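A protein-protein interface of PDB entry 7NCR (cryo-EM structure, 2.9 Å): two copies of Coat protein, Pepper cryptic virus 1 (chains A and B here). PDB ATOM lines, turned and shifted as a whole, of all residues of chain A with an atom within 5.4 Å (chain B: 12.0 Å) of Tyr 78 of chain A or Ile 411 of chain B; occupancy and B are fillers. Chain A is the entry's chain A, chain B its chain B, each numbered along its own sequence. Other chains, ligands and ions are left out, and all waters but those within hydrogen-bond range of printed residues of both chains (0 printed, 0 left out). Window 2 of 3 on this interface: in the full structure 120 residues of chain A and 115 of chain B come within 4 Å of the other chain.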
ATOM      1  N   ILE A  74      17.393  -0.530  24.732  1.00  0.00           N
ATOM      2  CA  ILE A  74      18.266  -1.174  25.704  1.00  0.00           C
ATOM      3  C   ILE A  74      19.049  -0.133  26.491  1.00  0.00           C
ATOM      4  O   ILE A  74      19.412  -0.367  27.648  1.00  0.00           O
ATOM      5  CB  ILE A  74      19.202  -2.177  25.003  1.00  0.00           C
ATOM      6  CG1 ILE A  74      18.424  -3.054  24.025  1.00  0.00           C
ATOM      7  CG2 ILE A  74      19.898  -3.057  26.019  1.00  0.00           C
ATOM      8  CD1 ILE A  74      17.518  -4.058  24.676  1.00  0.00           C
ATOM      9  N   PHE A  75      19.314   1.028  25.892  1.00  0.00           N
ATOM     10  CA  PHE A  75      20.016   2.078  26.620  1.00  0.00           C
ATOM     11  C   PHE A  75      19.116   2.797  27.615  1.00  0.00           C
ATOM     12  O   PHE A  75      19.586   3.192  28.683  1.00  0.00           O
ATOM     13  CB  PHE A  75      20.624   3.094  25.651  1.00  0.00           C
ATOM     14  CG  PHE A  75      21.821   2.583  24.909  1.00  0.00           C
ATOM     15  CD1 PHE A  75      22.704   1.709  25.511  1.00  0.00           C
ATOM     16  CD2 PHE A  75      22.065   2.976  23.607  1.00  0.00           C
ATOM     17  CE1 PHE A  75      23.805   1.236  24.824  1.00  0.00           C
ATOM     18  CE2 PHE A  75      23.161   2.504  22.922  1.00  0.00           C
ATOM     19  CZ  PHE A  75      24.030   1.635  23.531  1.00  0.00           C
ATOM     20  N   SER A  76      17.833   2.982  27.299  1.00  0.00           N
ATOM     21  CA  SER A  76      16.981   3.740  28.209  1.00  0.00           C
ATOM     22  C   SER A  76      16.544   2.922  29.416  1.00  0.00           C
ATOM     23  O   SER A  76      16.208   3.500  30.453  1.00  0.00           O
ATOM     24  CB  SER A  76      15.762   4.295  27.474  1.00  0.00           C
ATOM     25  OG  SER A  76      14.856   3.275  27.121  1.00  0.00           O
ATOM     26  N   SER A  77      16.538   1.596  29.321  1.00  0.00           N
ATOM     27  CA  SER A  77      16.249   0.787  30.494  1.00  0.00           C
ATOM     28  C   SER A  77      17.436   0.665  31.437  1.00  0.00           C
ATOM     29  O   SER A  77      17.284   0.117  32.531  1.00  0.00           O
ATOM     30  CB  SER A  77      15.783  -0.606  30.082  1.00  0.00           C
ATOM     31  OG  SER A  77      16.467  -1.051  28.936  1.00  0.00           O
ATOM     32  N   TYR A  78      18.609   1.153  31.047  1.00  0.00           N
ATOM     33  CA  TYR A  78      19.779   1.173  31.912  1.00  0.00           C
ATOM     34  C   TYR A  78      20.358   2.574  32.011  1.00  0.00           C
ATOM     35  O   TYR A  78      21.565   2.741  32.154  1.00  0.00           O
ATOM     36  CB  TYR A  78      20.840   0.197  31.418  1.00  0.00           C
ATOM     37  CG  TYR A  78      20.473  -1.246  31.620  1.00  0.00           C
ATOM     38  CD1 TYR A  78      19.861  -1.969  30.613  1.00  0.00           C
ATOM     39  CD2 TYR A  78      20.739  -1.883  32.818  1.00  0.00           C
ATOM     40  CE1 TYR A  78      19.524  -3.283  30.795  1.00  0.00           C
ATOM     41  CE2 TYR A  78      20.406  -3.198  33.007  1.00  0.00           C
ATOM     42  CZ  TYR A  78      19.796  -3.893  31.995  1.00  0.00           C
ATOM     43  OH  TYR A  78      19.464  -5.211  32.188  1.00  0.00           O
ATOM     44  N   TRP A  79      19.501   3.589  31.959  1.00  0.00           N
ATOM     45  CA  TRP A  79      19.982   4.946  31.763  1.00  0.00           C
ATOM     46  C   TRP A  79      20.680   5.520  32.986  1.00  0.00           C
ATOM     47  O   TRP A  79      21.427   6.490  32.850  1.00  0.00           O
ATOM     48  CB  TRP A  79      18.831   5.859  31.355  1.00  0.00           C
ATOM     49  CG  TRP A  79      19.317   7.142  30.814  1.00  0.00           C
ATOM     50  CD1 TRP A  79      19.078   8.380  31.311  1.00  0.00           C
ATOM     51  CD2 TRP A  79      20.164   7.321  29.678  1.00  0.00           C
ATOM     52  NE1 TRP A  79      19.711   9.325  30.552  1.00  0.00           N
ATOM     53  CE2 TRP A  79      20.386   8.698  29.540  1.00  0.00           C
ATOM     54  CE3 TRP A  79      20.749   6.449  28.757  1.00  0.00           C
ATOM     55  CZ2 TRP A  79      21.167   9.225  28.523  1.00  0.00           C
ATOM     56  CZ3 TRP A  79      21.524   6.976  27.750  1.00  0.00           C
ATOM     57  CH2 TRP A  79      21.725   8.350  27.639  1.00  0.00           C
ATOM     58  N   GLN A  80      20.453   4.959  34.172  1.00  0.00           N
ATOM     59  CA  GLN A  80      21.153   5.445  35.354  1.00  0.00           C
ATOM     60  C   GLN A  80      22.657   5.304  35.204  1.00  0.00           C
ATOM     61  O   GLN A  80      23.418   6.074  35.798  1.00  0.00           O
ATOM     62  CB  GLN A  80      20.690   4.688  36.593  1.00  0.00           C
ATOM     63  CG  GLN A  80      19.362   4.005  36.432  1.00  0.00           C
ATOM     64  CD  GLN A  80      19.508   2.577  35.995  1.00  0.00           C
ATOM     65  OE1 GLN A  80      20.505   1.928  36.291  1.00  0.00           O
ATOM     66  NE2 GLN A  80      18.512   2.072  35.287  1.00  0.00           N
ATOM     67  N   HIS A  81      23.100   4.324  34.424  1.00  0.00           N
ATOM     68  CA  HIS A  81      24.512   4.046  34.241  1.00  0.00           C
ATOM     69  C   HIS A  81      25.152   4.893  33.158  1.00  0.00           C
ATOM     70  O   HIS A  81      26.381   4.909  33.061  1.00  0.00           O
ATOM     71  CB  HIS A  81      24.703   2.564  33.921  1.00  0.00           C
ATOM     72  CG  HIS A  81      24.058   1.650  34.913  1.00  0.00           C
ATOM     73  ND1 HIS A  81      24.300   1.734  36.267  1.00  0.00           N
ATOM     74  CD2 HIS A  81      23.178   0.637  34.751  1.00  0.00           C
ATOM     75  CE1 HIS A  81      23.596   0.811  36.896  1.00  0.00           C
ATOM     76  NE2 HIS A  81      22.908   0.130  35.997  1.00  0.00           N
ATOM     77  N   PHE A  82      24.359   5.595  32.353  1.00  0.00           N
ATOM     78  CA  PHE A  82      24.877   6.458  31.303  1.00  0.00           C
ATOM     79  C   PHE A  82      24.521   7.919  31.509  1.00  0.00           C
ATOM     80  O   PHE A  82      24.926   8.756  30.700  1.00  0.00           O
ATOM     81  CB  PHE A  82      24.359   6.016  29.928  1.00  0.00           C
ATOM     82  CG  PHE A  82      24.439   4.538  29.689  1.00  0.00           C
ATOM     83  CD1 PHE A  82      25.641   3.937  29.382  1.00  0.00           C
ATOM     84  CD2 PHE A  82      23.308   3.753  29.766  1.00  0.00           C
ATOM     85  CE1 PHE A  82      25.710   2.582  29.160  1.00  0.00           C
ATOM     86  CE2 PHE A  82      23.372   2.403  29.546  1.00  0.00           C
ATOM     87  CZ  PHE A  82      24.571   1.814  29.243  1.00  0.00           C
ATOM     88  N   LYS A 212      28.463  -4.819  34.857  1.00  0.00           N
ATOM     89  CA  LYS A 212      28.278  -6.260  34.740  1.00  0.00           C
ATOM     90  C   LYS A 212      26.979  -6.636  34.041  1.00  0.00           C
ATOM     91  O   LYS A 212      26.761  -7.822  33.774  1.00  0.00           O
ATOM     92  CB  LYS A 212      28.313  -6.915  36.121  1.00  0.00           C
ATOM     93  CG  LYS A 212      27.026  -6.736  36.902  1.00  0.00           C
ATOM     94  CD  LYS A 212      26.981  -7.603  38.140  1.00  0.00           C
ATOM     95  CE  LYS A 212      25.738  -7.301  38.959  1.00  0.00           C
ATOM     96  NZ  LYS A 212      25.668  -8.108  40.209  1.00  0.00           N
ATOM     97  N   GLU A 213      26.113  -5.667  33.748  1.00  0.00           N
ATOM     98  CA  GLU A 213      24.882  -5.961  33.023  1.00  0.00           C
ATOM     99  C   GLU A 213      25.166  -6.236  31.558  1.00  0.00           C
ATOM    100  O   GLU A 213      24.533  -7.103  30.950  1.00  0.00           O
ATOM    101  CB  GLU A 213      23.889  -4.799  33.133  1.00  0.00           C
ATOM    102  CG  GLU A 213      23.432  -4.394  34.531  1.00  0.00           C
ATOM    103  CD  GLU A 213      24.553  -3.898  35.430  1.00  0.00           C
ATOM    104  OE1 GLU A 213      24.863  -4.579  36.425  1.00  0.00           O
ATOM    105  OE2 GLU A 213      25.127  -2.830  35.140  1.00  0.00           O
ATOM    106  N   PHE A 214      26.119  -5.514  30.986  1.00  0.00           N
ATOM    107  CA  PHE A 214      26.359  -5.501  29.555  1.00  0.00           C
ATOM    108  C   PHE A 214      27.557  -6.371  29.213  1.00  0.00           C
ATOM    109  O   PHE A 214      28.588  -6.321  29.887  1.00  0.00           O
ATOM    110  CB  PHE A 214      26.599  -4.072  29.070  1.00  0.00           C
ATOM    111  CG  PHE A 214      25.391  -3.197  29.160  1.00  0.00           C
ATOM    112  CD1 PHE A 214      25.038  -2.603  30.355  1.00  0.00           C
ATOM    113  CD2 PHE A 214      24.604  -2.965  28.049  1.00  0.00           C
ATOM    114  CE1 PHE A 214      23.926  -1.803  30.443  1.00  0.00           C
ATOM    115  CE2 PHE A 214      23.493  -2.161  28.131  1.00  0.00           C
ATOM    116  CZ  PHE A 214      23.153  -1.580  29.329  1.00  0.00           C
ATOM    117  N   LYS A 215      27.409  -7.171  28.169  1.00  0.00           N
ATOM    118  CA  LYS A 215      28.487  -7.997  27.657  1.00  0.00           C
ATOM    119  C   LYS A 215      29.169  -7.304  26.489  1.00  0.00           C
ATOM    120  O   LYS A 215      28.596  -6.437  25.828  1.00  0.00           O
ATOM    121  CB  LYS A 215      27.962  -9.361  27.213  1.00  0.00           C
ATOM    122  CG  LYS A 215      27.151 -10.077  28.257  1.00  0.00           C
ATOM    123  CD  LYS A 215      26.631 -11.382  27.718  1.00  0.00           C
ATOM    124  CE  LYS A 215      25.662 -12.016  28.675  1.00  0.00           C
ATOM    125  NZ  LYS A 215      24.997 -13.189  28.060  1.00  0.00           N
ATOM    126  N   LEU B  29      23.828 -17.359  20.296  1.00  0.00           N
ATOM    127  CA  LEU B  29      22.590 -16.760  19.808  1.00  0.00           C
ATOM    128  C   LEU B  29      21.461 -17.788  19.773  1.00  0.00           C
ATOM    129  O   LEU B  29      20.431 -17.568  19.144  1.00  0.00           O
ATOM    130  CB  LEU B  29      22.807 -16.151  18.419  1.00  0.00           C
ATOM    131  CG  LEU B  29      21.844 -15.071  17.922  1.00  0.00           C
ATOM    132  CD1 LEU B  29      21.358 -14.203  19.061  1.00  0.00           C
ATOM    133  CD2 LEU B  29      22.494 -14.221  16.852  1.00  0.00           C
ATOM    134  N   ARG B  31      19.831 -19.128  22.565  1.00  0.00           N
ATOM    135  CA  ARG B  31      18.754 -18.869  23.513  1.00  0.00           C
ATOM    136  C   ARG B  31      17.689 -17.973  22.894  1.00  0.00           C
ATOM    137  O   ARG B  31      16.490 -18.232  23.036  1.00  0.00           O
ATOM    138  CB  ARG B  31      19.317 -18.245  24.786  1.00  0.00           C
ATOM    139  CG  ARG B  31      18.533 -18.591  26.037  1.00  0.00           C
ATOM    140  CD  ARG B  31      18.943 -17.733  27.217  1.00  0.00           C
ATOM    141  NE  ARG B  31      20.375 -17.818  27.483  1.00  0.00           N
ATOM    142  CZ  ARG B  31      21.223 -16.804  27.348  1.00  0.00           C
ATOM    143  NH1 ARG B  31      20.789 -15.618  26.951  1.00  0.00           N
ATOM    144  NH2 ARG B  31      22.508 -16.977  27.613  1.00  0.00           N
ATOM    145  N   SER B  32      18.110 -16.927  22.182  1.00  0.00           N
ATOM    146  CA  SER B  32      17.164 -16.073  21.477  1.00  0.00           C
ATOM    147  C   SER B  32      16.462 -16.835  20.358  1.00  0.00           C
ATOM    148  O   SER B  32      15.266 -16.641  20.120  1.00  0.00           O
ATOM    149  CB  SER B  32      17.888 -14.851  20.921  1.00  0.00           C
ATOM    150  OG  SER B  32      18.745 -14.296  21.896  1.00  0.00           O
ATOM    151  N   ASN B 400       8.377  -6.120  20.253  1.00  0.00           N
ATOM    152  CA  ASN B 400       8.641  -6.652  21.583  1.00  0.00           C
ATOM    153  C   ASN B 400       9.486  -7.912  21.519  1.00  0.00           C
ATOM    154  O   ASN B 400      10.395  -8.096  22.334  1.00  0.00           O
ATOM    155  CB  ASN B 400       7.329  -6.911  22.319  1.00  0.00           C
ATOM    156  CG  ASN B 400       6.862  -5.704  23.103  1.00  0.00           C
ATOM    157  OD1 ASN B 400       6.332  -4.749  22.541  1.00  0.00           O
ATOM    158  ND2 ASN B 400       7.073  -5.735  24.411  1.00  0.00           N
ATOM    159  N   SER B 401       9.222  -8.789  20.552  1.00  0.00           N
ATOM    160  CA  SER B 401      10.030  -9.998  20.437  1.00  0.00           C
ATOM    161  C   SER B 401      11.425  -9.695  19.907  1.00  0.00           C
ATOM    162  O   SER B 401      12.389 -10.345  20.318  1.00  0.00           O
ATOM    163  CB  SER B 401       9.325 -11.024  19.558  1.00  0.00           C
ATOM    164  OG  SER B 401       8.581 -10.384  18.545  1.00  0.00           O
ATOM    165  N   ARG B 402      11.559  -8.702  19.020  1.00  0.00           N
ATOM    166  CA  ARG B 402      12.889  -8.262  18.603  1.00  0.00           C
ATOM    167  C   ARG B 402      13.699  -7.789  19.799  1.00  0.00           C
ATOM    168  O   ARG B 402      14.856  -8.187  19.983  1.00  0.00           O
ATOM    169  CB  ARG B 402      12.788  -7.142  17.567  1.00  0.00           C
ATOM    170  CG  ARG B 402      11.902  -7.437  16.391  1.00  0.00           C
ATOM    171  CD  ARG B 402      12.350  -6.698  15.145  1.00  0.00           C
ATOM    172  NE  ARG B 402      12.243  -5.249  15.263  1.00  0.00           N
ATOM    173  CZ  ARG B 402      13.267  -4.410  15.139  1.00  0.00           C
ATOM    174  NH1 ARG B 402      14.481  -4.868  14.903  1.00  0.00           N
ATOM    175  NH2 ARG B 402      13.075  -3.109  15.254  1.00  0.00           N
ATOM    176  N   THR B 403      13.098  -6.944  20.633  1.00  0.00           N
ATOM    177  CA  THR B 403      13.814  -6.416  21.781  1.00  0.00           C
ATOM    178  C   THR B 403      14.092  -7.497  22.817  1.00  0.00           C
ATOM    179  O   THR B 403      15.156  -7.490  23.436  1.00  0.00           O
ATOM    180  CB  THR B 403      13.032  -5.258  22.386  1.00  0.00           C
ATOM    181  OG1 THR B 403      12.923  -4.211  21.418  1.00  0.00           O
ATOM    182  CG2 THR B 403      13.739  -4.714  23.596  1.00  0.00           C
ATOM    183  N   ALA B 404      13.178  -8.449  23.000  1.00  0.00           N
ATOM    184  CA  ALA B 404      13.436  -9.538  23.935  1.00  0.00           C
ATOM    185  C   ALA B 404      14.563 -10.442  23.456  1.00  0.00           C
ATOM    186  O   ALA B 404      15.397 -10.871  24.261  1.00  0.00           O
ATOM    187  CB  ALA B 404      12.164 -10.349  24.153  1.00  0.00           C
ATOM    188  N   ALA B 405      14.610 -10.734  22.153  1.00  0.00           N
ATOM    189  CA  ALA B 405      15.687 -11.541  21.598  1.00  0.00           C
ATOM    190  C   ALA B 405      17.029 -10.826  21.655  1.00  0.00           C
ATOM    191  O   ALA B 405      18.059 -11.476  21.856  1.00  0.00           O
ATOM    192  CB  ALA B 405      15.351 -11.926  20.159  1.00  0.00           C
ATOM    193  N   LEU B 406      17.044  -9.505  21.477  1.00  0.00           N
ATOM    194  CA  LEU B 406      18.283  -8.761  21.655  1.00  0.00           C
ATOM    195  C   LEU B 406      18.692  -8.703  23.120  1.00  0.00           C
ATOM    196  O   LEU B 406      19.885  -8.787  23.443  1.00  0.00           O
ATOM    197  CB  LEU B 406      18.125  -7.353  21.093  1.00  0.00           C
ATOM    198  CG  LEU B 406      19.348  -6.450  21.178  1.00  0.00           C
ATOM    199  CD1 LEU B 406      20.494  -7.097  20.461  1.00  0.00           C
ATOM    200  CD2 LEU B 406      19.052  -5.092  20.590  1.00  0.00           C
ATOM    201  N   ARG B 407      17.714  -8.590  24.014  1.00  0.00           N
ATOM    202  CA  ARG B 407      17.964  -8.392  25.431  1.00  0.00           C
ATOM    203  C   ARG B 407      18.493  -9.654  26.085  1.00  0.00           C
ATOM    204  O   ARG B 407      19.374  -9.583  26.943  1.00  0.00           O
ATOM    205  CB  ARG B 407      16.673  -7.926  26.097  1.00  0.00           C
ATOM    206  CG  ARG B 407      16.816  -7.365  27.480  1.00  0.00           C
ATOM    207  CD  ARG B 407      15.468  -6.939  28.013  1.00  0.00           C
ATOM    208  NE  ARG B 407      14.871  -5.877  27.214  1.00  0.00           N
ATOM    209  CZ  ARG B 407      15.134  -4.584  27.383  1.00  0.00           C
ATOM    210  NH1 ARG B 407      15.986  -4.199  28.321  1.00  0.00           N
ATOM    211  NH2 ARG B 407      14.549  -3.675  26.616  1.00  0.00           N
ATOM    212  N   MET B 408      17.976 -10.819  25.704  1.00  0.00           N
ATOM    213  CA  MET B 408      18.526 -12.044  26.271  1.00  0.00           C
ATOM    214  C   MET B 408      19.869 -12.413  25.666  1.00  0.00           C
ATOM    215  O   MET B 408      20.498 -13.369  26.126  1.00  0.00           O
ATOM    216  CB  MET B 408      17.550 -13.209  26.106  1.00  0.00           C
ATOM    217  CG  MET B 408      17.049 -13.445  24.706  1.00  0.00           C
ATOM    218  SD  MET B 408      15.518 -14.397  24.739  1.00  0.00           S
ATOM    219  CE  MET B 408      16.026 -15.762  25.771  1.00  0.00           C
ATOM    220  N   PHE B 409      20.326 -11.673  24.662  1.00  0.00           N
ATOM    221  CA  PHE B 409      21.609 -11.925  24.029  1.00  0.00           C
ATOM    222  C   PHE B 409      22.699 -11.018  24.586  1.00  0.00           C
ATOM    223  O   PHE B 409      23.787 -11.489  24.926  1.00  0.00           O
ATOM    224  CB  PHE B 409      21.489 -11.739  22.517  1.00  0.00           C
ATOM    225  CG  PHE B 409      22.706 -12.161  21.759  1.00  0.00           C
ATOM    226  CD1 PHE B 409      23.503 -13.190  22.220  1.00  0.00           C
ATOM    227  CD2 PHE B 409      23.054 -11.531  20.585  1.00  0.00           C
ATOM    228  CE1 PHE B 409      24.622 -13.577  21.527  1.00  0.00           C
ATOM    229  CE2 PHE B 409      24.168 -11.922  19.889  1.00  0.00           C
ATOM    230  CZ  PHE B 409      24.958 -12.945  20.363  1.00  0.00           C
ATOM    231  N   ILE B 410      22.424  -9.718  24.691  1.00  0.00           N
ATOM    232  CA  ILE B 410      23.458  -8.762  25.062  1.00  0.00           C
ATOM    233  C   ILE B 410      23.407  -8.372  26.529  1.00  0.00           C
ATOM    234  O   ILE B 410      24.245  -7.580  26.975  1.00  0.00           O
ATOM    235  CB  ILE B 410      23.392  -7.512  24.166  1.00  0.00           C
ATOM    236  CG1 ILE B 410      22.164  -6.671  24.498  1.00  0.00           C
ATOM    237  CG2 ILE B 410      23.391  -7.913  22.707  1.00  0.00           C
ATOM    238  CD1 ILE B 410      22.025  -5.464  23.628  1.00  0.00           C
ATOM    239  N   ILE B 411      22.463  -8.903  27.295  1.00  0.00           N
ATOM    240  CA  ILE B 411      22.410  -8.633  28.728  1.00  0.00           C
ATOM    241  C   ILE B 411      22.721  -9.900  29.510  1.00  0.00           C
ATOM    242  O   ILE B 411      23.657  -9.936  30.306  1.00  0.00           O
ATOM    243  CB  ILE B 411      21.049  -8.061  29.147  1.00  0.00           C
ATOM    244  CG1 ILE B 411      20.661  -6.883  28.254  1.00  0.00           C
ATOM    245  CG2 ILE B 411      21.081  -7.636  30.595  1.00  0.00           C
ATOM    246  CD1 ILE B 411      21.589  -5.707  28.362  1.00  0.00           C
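The backbone carbonyl oxygen (O) of Ile 74 of chain A lies within hydrogen-bond range of the side-chain hydroxyl (OG) of Ser 77 of chain A, 3.3 Å away.
Hydrophobic or aromatic side chains of chain B that line the printed part of chain A: Ile 411.
Among the printed residues, 10 pairs touch across the chains.
Among the printed residues, no Asp or Glu carboxylate lies within 4 Å of a Lys or Arg side-chain nitrogen of the other chain.
Among the printed residues, pairs that only touch across the chains: Ile 74 of chain A with Thr 403 of chain B (3.98 Å), Ile 74 of chain A with Arg 407 of chain B (3.6 Å), Ile 74 of chain A with Ile 411 of chain B (3.9 Å), Tyr 78 of chain A with Ile 411 of chain B (3.3 Å), Phe 214 of chain A with Ile 410 of chain B (3.9 Å), Lys 215 of chain A with Phe 409 of chain B (3.8 Å) and Lys 215 of chain A with Ile 411 of chain B (3.3 Å).
Of the printed residues of chain B, Ile 74 of chain A touches Thr 403 (3.98 Å), Arg 407 (3.6 Å) and Ile 411 (3.9 Å).
No residue of chain B comes within 4 Å of Ser 76 of chain A.
Of chain B, only Ile 411 (3.3 Å) comes within 4 Å of Tyr 78 of chain A.
No residue of chain B comes within 4 Å of Gln 80 of chain A.
No residue of chain B comes within 4 Å of Phe 82 of chain A.
Printed residues of chain B within 4 Å of Glu 213 of chain A: Ile 411.
Phe 214 of chain A touches one residue of chain B.
Lys 215 of chain A touches just these residues of chain B: Phe 409 (3.8 Å), Ile 410 (3.4 Å) and Ile 411 (3.3 Å).
Of the printed residues of chain A, Thr 403 of chain B touches Ile 74.
Ala 404 of chain B touches none of the printed residues of chain A.
Of the printed residues of chain A, Ile 410 of chain B touches Phe 214 and Lys 215.
Ile 411 of chain B touches just these residues of chain A: Ile 74, Tyr 78, Glu 213 and Lys 215.
No position is printed for both chains.
Of the 10 pairs that touch across the chains among the printed residues, none has its exchanged pair printed and touching as well.
The backbone carbonyl oxygen of Ile 410 of chain B lies within hydrogen-bond range of the backbone NH of Lys 215 of chain A (3.4 Å).
O of Glu 213 of chain A lies close to O of Ile 411 of chain B, at 3.0 Å.
The guanidinium group (NH1) of Arg 407 of chain B sits at hydrogen-bond distance from the side-chain hydroxyl (OG) of Ser 77 of chain A (3.2 Å).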
